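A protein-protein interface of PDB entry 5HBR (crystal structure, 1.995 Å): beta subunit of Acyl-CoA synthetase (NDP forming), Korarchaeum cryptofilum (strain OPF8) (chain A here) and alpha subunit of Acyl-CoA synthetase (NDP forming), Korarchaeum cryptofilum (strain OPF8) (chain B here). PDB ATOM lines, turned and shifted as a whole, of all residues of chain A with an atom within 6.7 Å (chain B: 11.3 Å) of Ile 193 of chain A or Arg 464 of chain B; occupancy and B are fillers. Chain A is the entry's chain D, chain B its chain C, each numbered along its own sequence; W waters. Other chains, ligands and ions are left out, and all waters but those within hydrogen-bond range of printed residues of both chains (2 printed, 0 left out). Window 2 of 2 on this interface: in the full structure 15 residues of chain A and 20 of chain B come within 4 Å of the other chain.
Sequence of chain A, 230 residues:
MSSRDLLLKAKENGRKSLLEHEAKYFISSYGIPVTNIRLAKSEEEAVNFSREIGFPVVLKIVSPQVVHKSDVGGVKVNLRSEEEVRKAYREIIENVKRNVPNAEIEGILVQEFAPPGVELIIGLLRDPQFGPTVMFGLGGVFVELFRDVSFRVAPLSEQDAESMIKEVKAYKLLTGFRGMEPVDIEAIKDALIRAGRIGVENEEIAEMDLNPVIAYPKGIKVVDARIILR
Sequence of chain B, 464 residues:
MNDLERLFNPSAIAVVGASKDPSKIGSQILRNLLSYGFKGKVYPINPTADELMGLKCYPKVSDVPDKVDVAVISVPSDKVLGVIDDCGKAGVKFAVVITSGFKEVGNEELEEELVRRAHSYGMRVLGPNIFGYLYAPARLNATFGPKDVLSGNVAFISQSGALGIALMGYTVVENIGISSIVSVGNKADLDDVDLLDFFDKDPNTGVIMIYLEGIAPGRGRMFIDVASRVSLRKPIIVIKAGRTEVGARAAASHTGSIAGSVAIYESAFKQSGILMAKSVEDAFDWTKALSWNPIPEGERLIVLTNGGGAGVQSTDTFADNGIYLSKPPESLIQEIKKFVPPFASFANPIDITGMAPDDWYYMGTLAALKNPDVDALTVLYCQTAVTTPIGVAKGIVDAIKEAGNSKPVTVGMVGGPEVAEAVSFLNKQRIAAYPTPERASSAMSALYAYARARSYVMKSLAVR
O of Ala 154 of chain A is in hydrogen-bond range of NH1 of Arg 221 of chain B (3.0 Å). The side-chain hydroxyl of Tyr 456 of chain B is in hydrogen-bond range of the side-chain carboxylate of Asp 160 of chain A, 2.7 Å away.
The backbone NH of Gln 159 of chain A lies close to the side-chain hydroxyl of Ser 157 of chain A. N of Ser 157 of chain A is in hydrogen-bond range of OD2 of Asp 160 of chain A, 2.8 Å away.
Among the printed residues, pairs that only touch across the chains: Pro 155 of chain A with Arg 221 of chain B, Ser 157 of chain A with Ser 460 of chain B, Gln 159 of chain A with Tyr 456 of chain B, Gln 159 of chain A with Lys 459 of chain B, Asp 160 of chain A with Gln 271 of chain B and Ile 193 of chain A with Arg 464 of chain B.
Of the printed residues of chain B, Ile 193 of chain A touches Arg 464 (3.8 Å). Of chain A, only Ile 193 (3.8 Å) comes within 4 Å of Arg 464 of chain B. No residue of chain B comes within 4 Å of Leu 156 of chain A. No residue of chain B comes within 4 Å of Lys 189 of chain A. No residue of chain B comes within 4 Å of Asp 190 of chain A. No residue of chain B comes within 4 Å of Ala 191 of chain A. No residue of chain B comes within 4 Å of Leu 192 of chain A. Printed residues of chain A within 4 Å of Tyr 456 of chain B: Gln 159 and Asp 160. Of the printed residues of chain B, Gln 159 of chain A touches Tyr 456 and Lys 459. Of the printed residues of chain A, Arg 221 of chain B touches Ala 154 (3.0 Å) and Pro 155 (3.6 Å). Of the printed residues of chain A, Lys 459 of chain B touches Gln 159. Of the printed residues of chain A, Ser 460 of chain B touches Ser 157. The nearest residue of chain A that does not touch Arg 464 of chain B is Leu 156 of chain A (4.1 Å). The nearest printed residue of chain A that does not touch Lys 459 of chain B is Ser 157 of chain A (4.9 Å).
Printed residues of chain B that touch a printed residue of chain A: Arg 221, Gln 271, Tyr 456, Lys 459, Ser 460 and Arg 464. Of the 21 printed residues of chain A, 6 touch a printed residue of chain B. Printed residues of chain A that touch a printed residue of chain B: Ala 154, Pro 155, Ser 157, Gln 159, Asp 160 and Ile 193. Along chain A the printed residues that touch a printed residue of chain B span positions 154 to 193. Among the printed residues, 8 pairs touch across the chains. Among the printed residues, no Asp or Glu carboxylate lies within 4 Å of a Lys or Arg side-chain nitrogen of the other chain.
Water W1 bridges OD2 of Asp 160 of chain A (2.6 Å) and NE2 of Gln 271 of chain B (3.3 Å). Water W2 lies within hydrogen-bond range of the backbone carbonyl oxygen of Lys 459 of chain B (2.6 Å), the backbone NH of Gln 159 of chain A (3.0 Å) and the backbone NH of Glu 158 of chain A (3.4 Å).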
ATOM      1  N   ILE A  32      31.293   5.281  18.804  1.00  0.00           N
ATOM      2  CA  ILE A  32      29.972   5.198  19.415  1.00  0.00           C
ATOM      3  C   ILE A  32      29.657   6.564  20.070  1.00  0.00           C
ATOM      4  O   ILE A  32      30.378   6.990  20.976  1.00  0.00           O
ATOM      5  CB  ILE A  32      29.893   4.066  20.447  1.00  0.00           C
ATOM      6  CG1 ILE A  32      30.149   2.718  19.757  1.00  0.00           C
ATOM      7  CG2 ILE A  32      28.531   4.067  21.103  1.00  0.00           C
ATOM      8  CD1 ILE A  32      30.076   1.517  20.666  1.00  0.00           C
ATOM      9  N   VAL A 134      27.640  -9.839  22.155  1.00  0.00           N
ATOM     10  CA  VAL A 134      26.910  -8.596  22.250  1.00  0.00           C
ATOM     11  C   VAL A 134      25.450  -8.897  22.551  1.00  0.00           C
ATOM     12  O   VAL A 134      24.878  -9.878  22.058  1.00  0.00           O
ATOM     13  CB  VAL A 134      27.034  -7.759  20.942  1.00  0.00           C
ATOM     14  CG1 VAL A 134      26.173  -6.505  20.999  1.00  0.00           C
ATOM     15  CG2 VAL A 134      28.494  -7.386  20.675  1.00  0.00           C
ATOM     16  N   ALA A 154      30.421 -12.136  18.810  1.00  0.00           N
ATOM     17  CA  ALA A 154      31.221 -11.175  18.044  1.00  0.00           C
ATOM     18  C   ALA A 154      32.384 -11.850  17.341  1.00  0.00           C
ATOM     19  O   ALA A 154      32.825 -12.914  17.771  1.00  0.00           O
ATOM     20  CB  ALA A 154      31.745 -10.049  18.984  1.00  0.00           C
ATOM     21  N   PRO A 155      32.904 -11.240  16.255  1.00  0.00           N
ATOM     22  CA  PRO A 155      32.493  -9.968  15.654  1.00  0.00           C
ATOM     23  C   PRO A 155      31.146 -10.073  14.948  1.00  0.00           C
ATOM     24  O   PRO A 155      30.802 -11.142  14.437  1.00  0.00           O
ATOM     25  CB  PRO A 155      33.602  -9.690  14.648  1.00  0.00           C
ATOM     26  CG  PRO A 155      34.022 -11.026  14.213  1.00  0.00           C
ATOM     27  CD  PRO A 155      33.949 -11.890  15.445  1.00  0.00           C
ATOM     28  N   LEU A 156      30.420  -8.964  14.905  1.00  0.00           N
ATOM     29  CA  LEU A 156      29.089  -8.916  14.311  1.00  0.00           C
ATOM     30  C   LEU A 156      29.082  -8.418  12.866  1.00  0.00           C
ATOM     31  O   LEU A 156      29.634  -7.368  12.563  1.00  0.00           O
ATOM     32  CB  LEU A 156      28.186  -8.004  15.135  1.00  0.00           C
ATOM     33  CG  LEU A 156      27.331  -8.652  16.212  1.00  0.00           C
ATOM     34  CD1 LEU A 156      28.199  -9.412  17.178  1.00  0.00           C
ATOM     35  CD2 LEU A 156      26.527  -7.596  16.924  1.00  0.00           C
ATOM     36  N   SER A 157      28.415  -9.158  11.988  1.00  0.00           N
ATOM     37  CA  SER A 157      28.146  -8.669  10.646  1.00  0.00           C
ATOM     38  C   SER A 157      26.953  -7.737  10.701  1.00  0.00           C
ATOM     39  O   SER A 157      26.236  -7.701  11.700  1.00  0.00           O
ATOM     40  CB  SER A 157      27.851  -9.820   9.690  1.00  0.00           C
ATOM     41  OG  SER A 157      26.663 -10.477  10.104  1.00  0.00           O
ATOM     42  N   GLU A 158      26.728  -7.013   9.610  1.00  0.00           N
ATOM     43  CA  GLU A 158      25.543  -6.178   9.450  1.00  0.00           C
ATOM     44  C   GLU A 158      24.267  -7.015   9.584  1.00  0.00           C
ATOM     45  O   GLU A 158      23.280  -6.578  10.160  1.00  0.00           O
ATOM     46  CB  GLU A 158      25.594  -5.472   8.096  1.00  0.00           C
ATOM     47  CG  GLU A 158      24.525  -4.410   7.906  1.00  0.00           C
ATOM     48  CD  GLU A 158      24.560  -3.766   6.524  1.00  0.00           C
ATOM     49  OE1 GLU A 158      25.643  -3.731   5.891  1.00  0.00           O
ATOM     50  OE2 GLU A 158      23.493  -3.297   6.071  1.00  0.00           O
ATOM     51  N   GLN A 159      24.302  -8.235   9.060  1.00  0.00           N
ATOM     52  CA  GLN A 159      23.191  -9.179   9.207  1.00  0.00           C
ATOM     53  C   GLN A 159      22.929  -9.538  10.671  1.00  0.00           C
ATOM     54  O   GLN A 159      21.780  -9.622  11.103  1.00  0.00           O
ATOM     55  CB  GLN A 159      23.486 -10.458   8.418  1.00  0.00           C
ATOM     56  CG  GLN A 159      22.424 -11.528   8.556  1.00  0.00           C
ATOM     57  CD  GLN A 159      21.122 -11.128   7.903  1.00  0.00           C
ATOM     58  OE1 GLN A 159      21.068 -10.163   7.152  1.00  0.00           O
ATOM     59  NE2 GLN A 159      20.066 -11.874   8.183  1.00  0.00           N
ATOM     60  N   ASP A 160      23.998  -9.778  11.425  1.00  0.00           N
ATOM     61  CA  ASP A 160      23.859 -10.100  12.840  1.00  0.00           C
ATOM     62  C   ASP A 160      23.157  -9.000  13.575  1.00  0.00           C
ATOM     63  O   ASP A 160      22.218  -9.254  14.322  1.00  0.00           O
ATOM     64  CB  ASP A 160      25.216 -10.334  13.498  1.00  0.00           C
ATOM     65  CG  ASP A 160      25.889 -11.580  13.014  1.00  0.00           C
ATOM     66  OD1 ASP A 160      25.195 -12.610  12.880  1.00  0.00           O
ATOM     67  OD2 ASP A 160      27.119 -11.519  12.763  1.00  0.00           O
ATOM     68  N   ALA A 161      23.628  -7.775  13.372  1.00  0.00           N
ATOM     69  CA  ALA A 161      23.063  -6.612  14.046  1.00  0.00           C
ATOM     70  C   ALA A 161      21.589  -6.425  13.681  1.00  0.00           C
ATOM     71  O   ALA A 161      20.732  -6.288  14.559  1.00  0.00           O
ATOM     72  CB  ALA A 161      23.862  -5.362  13.701  1.00  0.00           C
ATOM     73  N   ILE A 188      21.724   2.200  15.386  1.00  0.00           N
ATOM     74  CA  ILE A 188      21.761   1.147  16.389  1.00  0.00           C
ATOM     75  C   ILE A 188      22.680   0.009  15.911  1.00  0.00           C
ATOM     76  O   ILE A 188      23.555  -0.458  16.644  1.00  0.00           O
ATOM     77  CB  ILE A 188      20.344   0.615  16.689  1.00  0.00           C
ATOM     78  CG1 ILE A 188      19.458   1.741  17.233  1.00  0.00           C
ATOM     79  CG2 ILE A 188      20.393  -0.534  17.704  1.00  0.00           C
ATOM     80  CD1 ILE A 188      17.985   1.353  17.397  1.00  0.00           C
ATOM     81  N   LYS A 189      22.493  -0.409  14.666  1.00  0.00           N
ATOM     82  CA  LYS A 189      23.284  -1.473  14.080  1.00  0.00           C
ATOM     83  C   LYS A 189      24.763  -1.141  14.131  1.00  0.00           C
ATOM     84  O   LYS A 189      25.588  -1.972  14.521  1.00  0.00           O
ATOM     85  CB  LYS A 189      22.858  -1.710  12.640  1.00  0.00           C
ATOM     86  CG  LYS A 189      21.489  -2.366  12.507  1.00  0.00           C
ATOM     87  CD  LYS A 189      20.973  -2.312  11.071  1.00  0.00           C
ATOM     88  CE  LYS A 189      21.977  -2.895  10.074  1.00  0.00           C
ATOM     89  NZ  LYS A 189      21.503  -2.758   8.669  1.00  0.00           N
ATOM     90  N   ASP A 190      25.083   0.089  13.755  1.00  0.00           N
ATOM     91  CA  ASP A 190      26.448   0.569  13.787  1.00  0.00           C
ATOM     92  C   ASP A 190      27.064   0.451  15.193  1.00  0.00           C
ATOM     93  O   ASP A 190      28.218   0.031  15.349  1.00  0.00           O
ATOM     94  CB  ASP A 190      26.490   2.020  13.311  1.00  0.00           C
ATOM     95  CG  ASP A 190      27.864   2.618  13.410  1.00  0.00           C
ATOM     96  OD1 ASP A 190      28.717   2.268  12.567  1.00  0.00           O
ATOM     97  OD2 ASP A 190      28.099   3.435  14.333  1.00  0.00           O
ATOM     98  N   ALA A 191      26.297   0.817  16.214  1.00  0.00           N
ATOM     99  CA  ALA A 191      26.794   0.783  17.587  1.00  0.00           C
ATOM    100  C   ALA A 191      26.965  -0.651  18.090  1.00  0.00           C
ATOM    101  O   ALA A 191      27.907  -0.964  18.841  1.00  0.00           O
ATOM    102  CB  ALA A 191      25.863   1.542  18.491  1.00  0.00           C
ATOM    103  N   LEU A 192      26.039  -1.518  17.686  1.00  0.00           N
ATOM    104  CA  LEU A 192      26.113  -2.928  18.047  1.00  0.00           C
ATOM    105  C   LEU A 192      27.401  -3.521  17.501  1.00  0.00           C
ATOM    106  O   LEU A 192      28.130  -4.189  18.234  1.00  0.00           O
ATOM    107  CB  LEU A 192      24.895  -3.698  17.528  1.00  0.00           C
ATOM    108  CG  LEU A 192      23.624  -3.434  18.322  1.00  0.00           C
ATOM    109  CD1 LEU A 192      22.404  -3.931  17.584  1.00  0.00           C
ATOM    110  CD2 LEU A 192      23.729  -4.099  19.681  1.00  0.00           C
ATOM    111  N   ILE A 193      27.693  -3.249  16.233  1.00  0.00           N
ATOM    112  CA  ILE A 193      28.881  -3.799  15.572  1.00  0.00           C
ATOM    113  C   ILE A 193      30.150  -3.300  16.247  1.00  0.00           C
ATOM    114  O   ILE A 193      31.116  -4.054  16.432  1.00  0.00           O
ATOM    115  CB  ILE A 193      28.906  -3.432  14.069  1.00  0.00           C
ATOM    116  CG1 ILE A 193      27.772  -4.167  13.344  1.00  0.00           C
ATOM    117  CG2 ILE A 193      30.256  -3.790  13.426  1.00  0.00           C
ATOM    118  CD1 ILE A 193      27.476  -3.623  11.969  1.00  0.00           C
ATOM    119  N   ARG A 194      30.145  -2.027  16.616  1.00  0.00           N
ATOM    120  CA  ARG A 194      31.303  -1.416  17.249  1.00  0.00           C
ATOM    121  C   ARG A 194      31.492  -1.933  18.664  1.00  0.00           C
ATOM    122  O   ARG A 194      32.628  -2.137  19.108  1.00  0.00           O
ATOM    123  CB  ARG A 194      31.165   0.109  17.237  1.00  0.00           C
ATOM    124  CG  ARG A 194      31.315   0.693  15.834  1.00  0.00           C
ATOM    125  CD  ARG A 194      30.995   2.176  15.790  1.00  0.00           C
ATOM    126  NE  ARG A 194      30.936   2.678  14.419  1.00  0.00           N
ATOM    127  CZ  ARG A 194      31.985   3.069  13.701  1.00  0.00           C
ATOM    128  NH1 ARG A 194      33.212   3.027  14.206  1.00  0.00           N
ATOM    129  NH2 ARG A 194      31.806   3.503  12.461  1.00  0.00           N
ATOM    130  N   ALA A 195      30.394  -2.159  19.378  1.00  0.00           N
ATOM    131  CA  ALA A 195      30.464  -2.800  20.690  1.00  0.00           C
ATOM    132  C   ALA A 195      31.124  -4.166  20.565  1.00  0.00           C
ATOM    133  O   ALA A 195      31.969  -4.542  21.370  1.00  0.00           O
ATOM    134  CB  ALA A 195      29.087  -2.926  21.295  1.00  0.00           C
ATOM    135  N   GLY A 196      30.766  -4.905  19.531  1.00  0.00           N
ATOM    136  CA  GLY A 196      31.351  -6.217  19.332  1.00  0.00           C
ATOM    137  C   GLY A 196      32.841  -6.119  19.051  1.00  0.00           C
ATOM    138  O   GLY A 196      33.633  -6.968  19.473  1.00  0.00           O
ATOM    139  N   ARG A 197      33.227  -5.067  18.345  1.00  0.00           N
ATOM    140  CA  ARG A 197      34.620  -4.874  17.998  1.00  0.00           C
ATOM    141  C   ARG A 197      35.439  -4.554  19.248  1.00  0.00           C
ATOM    142  O   ARG A 197      36.564  -5.015  19.382  1.00  0.00           O
ATOM    143  CB  ARG A 197      34.755  -3.769  16.965  1.00  0.00           C
ATOM    144  CG  ARG A 197      36.127  -3.666  16.357  1.00  0.00           C
ATOM    145  CD  ARG A 197      36.248  -2.419  15.488  1.00  0.00           C
ATOM    146  NE  ARG A 197      37.529  -2.382  14.778  1.00  0.00           N
ATOM    147  CZ  ARG A 197      37.792  -1.594  13.740  1.00  0.00           C
ATOM    148  NH1 ARG A 197      36.868  -0.766  13.269  1.00  0.00           N
ATOM    149  NH2 ARG A 197      38.983  -1.644  13.161  1.00  0.00           N
ATOM    150  N   ILE A 198      34.860  -3.780  20.164  1.00  0.00           N
ATOM    151  CA  ILE A 198      35.508  -3.444  21.434  1.00  0.00           C
ATOM    152  C   ILE A 198      35.850  -4.703  22.234  1.00  0.00           C
ATOM    153  O   ILE A 198      36.923  -4.808  22.836  1.00  0.00           O
ATOM    154  CB  ILE A 198      34.601  -2.527  22.289  1.00  0.00           C
ATOM    155  CG1 ILE A 198      34.660  -1.093  21.770  1.00  0.00           C
ATOM    156  CG2 ILE A 198      35.015  -2.550  23.776  1.00  0.00           C
ATOM    157  CD1 ILE A 198      33.576  -0.192  22.337  1.00  0.00           C
ATOM    158  N   ARG B 221      33.832 -19.975  19.134  1.00  0.00           N
ATOM    159  CA  ARG B 221      34.085 -19.108  17.990  1.00  0.00           C
ATOM    160  C   ARG B 221      34.475 -19.941  16.776  1.00  0.00           C
ATOM    161  O   ARG B 221      33.913 -19.774  15.682  1.00  0.00           O
ATOM    162  CB  ARG B 221      35.184 -18.093  18.315  1.00  0.00           C
ATOM    163  CG  ARG B 221      35.447 -17.072  17.220  1.00  0.00           C
ATOM    164  CD  ARG B 221      34.224 -16.205  16.944  1.00  0.00           C
ATOM    165  NE  ARG B 221      33.659 -16.477  15.628  1.00  0.00           N
ATOM    166  CZ  ARG B 221      32.592 -15.867  15.110  1.00  0.00           C
ATOM    167  NH1 ARG B 221      31.944 -14.921  15.783  1.00  0.00           N
ATOM    168  NH2 ARG B 221      32.167 -16.204  13.902  1.00  0.00           N
ATOM    169  N   GLN B 271      23.860 -18.111  13.913  1.00  0.00           N
ATOM    170  CA  GLN B 271      24.982 -17.519  13.182  1.00  0.00           C
ATOM    171  C   GLN B 271      25.737 -18.572  12.349  1.00  0.00           C
ATOM    172  O   GLN B 271      26.428 -18.234  11.393  1.00  0.00           O
ATOM    173  CB  GLN B 271      25.942 -16.820  14.153  1.00  0.00           C
ATOM    174  CG  GLN B 271      25.339 -15.582  14.827  1.00  0.00           C
ATOM    175  CD  GLN B 271      26.243 -14.990  15.897  1.00  0.00           C
ATOM    176  OE1 GLN B 271      25.994 -15.154  17.089  1.00  0.00           O
ATOM    177  NE2 GLN B 271      27.283 -14.290  15.476  1.00  0.00           N
ATOM    178  N   TYR B 456      21.129 -16.594   5.677  1.00  0.00           N
ATOM    179  CA  TYR B 456      21.613 -15.838   6.830  1.00  0.00           C
ATOM    180  C   TYR B 456      23.148 -15.844   6.842  1.00  0.00           C
ATOM    181  O   TYR B 456      23.787 -14.825   7.085  1.00  0.00           O
ATOM    182  CB  TYR B 456      21.086 -16.418   8.148  1.00  0.00           C
ATOM    183  CG  TYR B 456      21.494 -15.604   9.373  1.00  0.00           C
ATOM    184  CD1 TYR B 456      22.793 -15.638   9.857  1.00  0.00           C
ATOM    185  CD2 TYR B 456      20.574 -14.806  10.035  1.00  0.00           C
ATOM    186  CE1 TYR B 456      23.176 -14.878  10.962  1.00  0.00           C
ATOM    187  CE2 TYR B 456      20.934 -14.053  11.153  1.00  0.00           C
ATOM    188  CZ  TYR B 456      22.235 -14.093  11.607  1.00  0.00           C
ATOM    189  OH  TYR B 456      22.603 -13.344  12.708  1.00  0.00           O
ATOM    190  N   MET B 458      25.244 -16.513   4.250  1.00  0.00           N
ATOM    191  CA  MET B 458      25.772 -15.827   3.084  1.00  0.00           C
ATOM    192  C   MET B 458      25.798 -14.316   3.328  1.00  0.00           C
ATOM    193  O   MET B 458      26.826 -13.679   3.117  1.00  0.00           O
ATOM    194  CB  MET B 458      24.961 -16.177   1.838  1.00  0.00           C
ATOM    195  CG  MET B 458      25.265 -17.585   1.289  1.00  0.00           C
ATOM    196  SD  MET B 458      24.429 -18.044  -0.266  1.00  0.00           S
ATOM    197  CE  MET B 458      22.692 -18.026   0.199  1.00  0.00           C
ATOM    198  N   LYS B 459      24.695 -13.764   3.826  1.00  0.00           N
ATOM    199  CA  LYS B 459      24.626 -12.341   4.138  1.00  0.00           C
ATOM    200  C   LYS B 459      25.599 -11.919   5.239  1.00  0.00           C
ATOM    201  O   LYS B 459      26.089 -10.788   5.228  1.00  0.00           O
ATOM    202  CB  LYS B 459      23.223 -11.952   4.560  1.00  0.00           C
ATOM    203  CG  LYS B 459      22.159 -12.133   3.480  1.00  0.00           C
ATOM    204  CD  LYS B 459      20.857 -11.481   3.920  1.00  0.00           C
ATOM    205  CE  LYS B 459      19.655 -12.058   3.211  1.00  0.00           C
ATOM    206  NZ  LYS B 459      19.212 -13.323   3.878  1.00  0.00           N
ATOM    207  N   SER B 460      25.875 -12.801   6.196  1.00  0.00           N
ATOM    208  CA  SER B 460      26.779 -12.428   7.281  1.00  0.00           C
ATOM    209  C   SER B 460      28.226 -12.413   6.797  1.00  0.00           C
ATOM    210  O   SER B 460      29.041 -11.679   7.345  1.00  0.00           O
ATOM    211  CB  SER B 460      26.640 -13.369   8.491  1.00  0.00           C
ATOM    212  OG  SER B 460      27.189 -14.654   8.217  1.00  0.00           O
ATOM    213  N   LEU B 461      28.536 -13.221   5.783  1.00  0.00           N
ATOM    214  CA  LEU B 461      29.899 -13.313   5.234  1.00  0.00           C
ATOM    215  C   LEU B 461      30.117 -12.332   4.095  1.00  0.00           C
ATOM    216  O   LEU B 461      31.159 -12.354   3.436  1.00  0.00           O
ATOM    217  CB  LEU B 461      30.196 -14.724   4.726  1.00  0.00           C
ATOM    218  CG  LEU B 461      30.066 -15.844   5.739  1.00  0.00           C
ATOM    219  CD1 LEU B 461      30.258 -17.181   5.025  1.00  0.00           C
ATOM    220  CD2 LEU B 461      31.073 -15.668   6.864  1.00  0.00           C
ATOM    221  N   ALA B 462      29.125 -11.484   3.853  1.00  0.00           N
ATOM    222  CA  ALA B 462      29.233 -10.461   2.829  1.00  0.00           C
ATOM    223  C   ALA B 462      30.517  -9.640   3.003  1.00  0.00           C
ATOM    224  O   ALA B 462      30.909  -9.301   4.123  1.00  0.00           O
ATOM    225  CB  ALA B 462      28.004  -9.549   2.862  1.00  0.00           C
ATOM    226  N   VAL B 463      31.179  -9.346   1.887  1.00  0.00           N
ATOM    227  CA  VAL B 463      32.356  -8.482   1.879  1.00  0.00           C
ATOM    228  C   VAL B 463      31.911  -7.030   2.033  1.00  0.00           C
ATOM    229  O   VAL B 463      30.931  -6.606   1.416  1.00  0.00           O
ATOM    230  CB  VAL B 463      33.182  -8.659   0.572  1.00  0.00           C
ATOM    231  CG1 VAL B 463      34.285  -7.593   0.451  1.00  0.00           C
ATOM    232  CG2 VAL B 463      33.769 -10.069   0.505  1.00  0.00           C
ATOM    233  N   ARG B 464      32.635  -6.288   2.866  1.00  0.00           N
ATOM    234  CA  ARG B 464      32.368  -4.870   3.111  1.00  0.00           C
ATOM    235  C   ARG B 464      32.927  -3.974   2.006  1.00  0.00           C
ATOM    236  O   ARG B 464      33.911  -4.310   1.337  1.00  0.00           O
ATOM    237  CB  ARG B 464      32.973  -4.436   4.446  1.00  0.00           C
ATOM    238  CG  ARG B 464      32.383  -5.115   5.661  1.00  0.00           C
ATOM    239  CD  ARG B 464      33.215  -4.795   6.891  1.00  0.00           C
ATOM    240  NE  ARG B 464      32.475  -4.995   8.133  1.00  0.00           N
ATOM    241  CZ  ARG B 464      32.990  -4.806   9.343  1.00  0.00           C
ATOM    242  NH1 ARG B 464      34.254  -4.417   9.476  1.00  0.00           N
ATOM    243  NH2 ARG B 464      32.243  -5.008  10.424  1.00  0.00           N
ATOM    244  OXT ARG B 464      32.415  -2.875   1.779  1.00  0.00           O
HETATM  245  O   HOH W   1      27.733 -14.001  12.174  1.00  0.00           O
HETATM  246  O   HOH W   2      26.120  -8.617   6.727  1.00  0.00           O
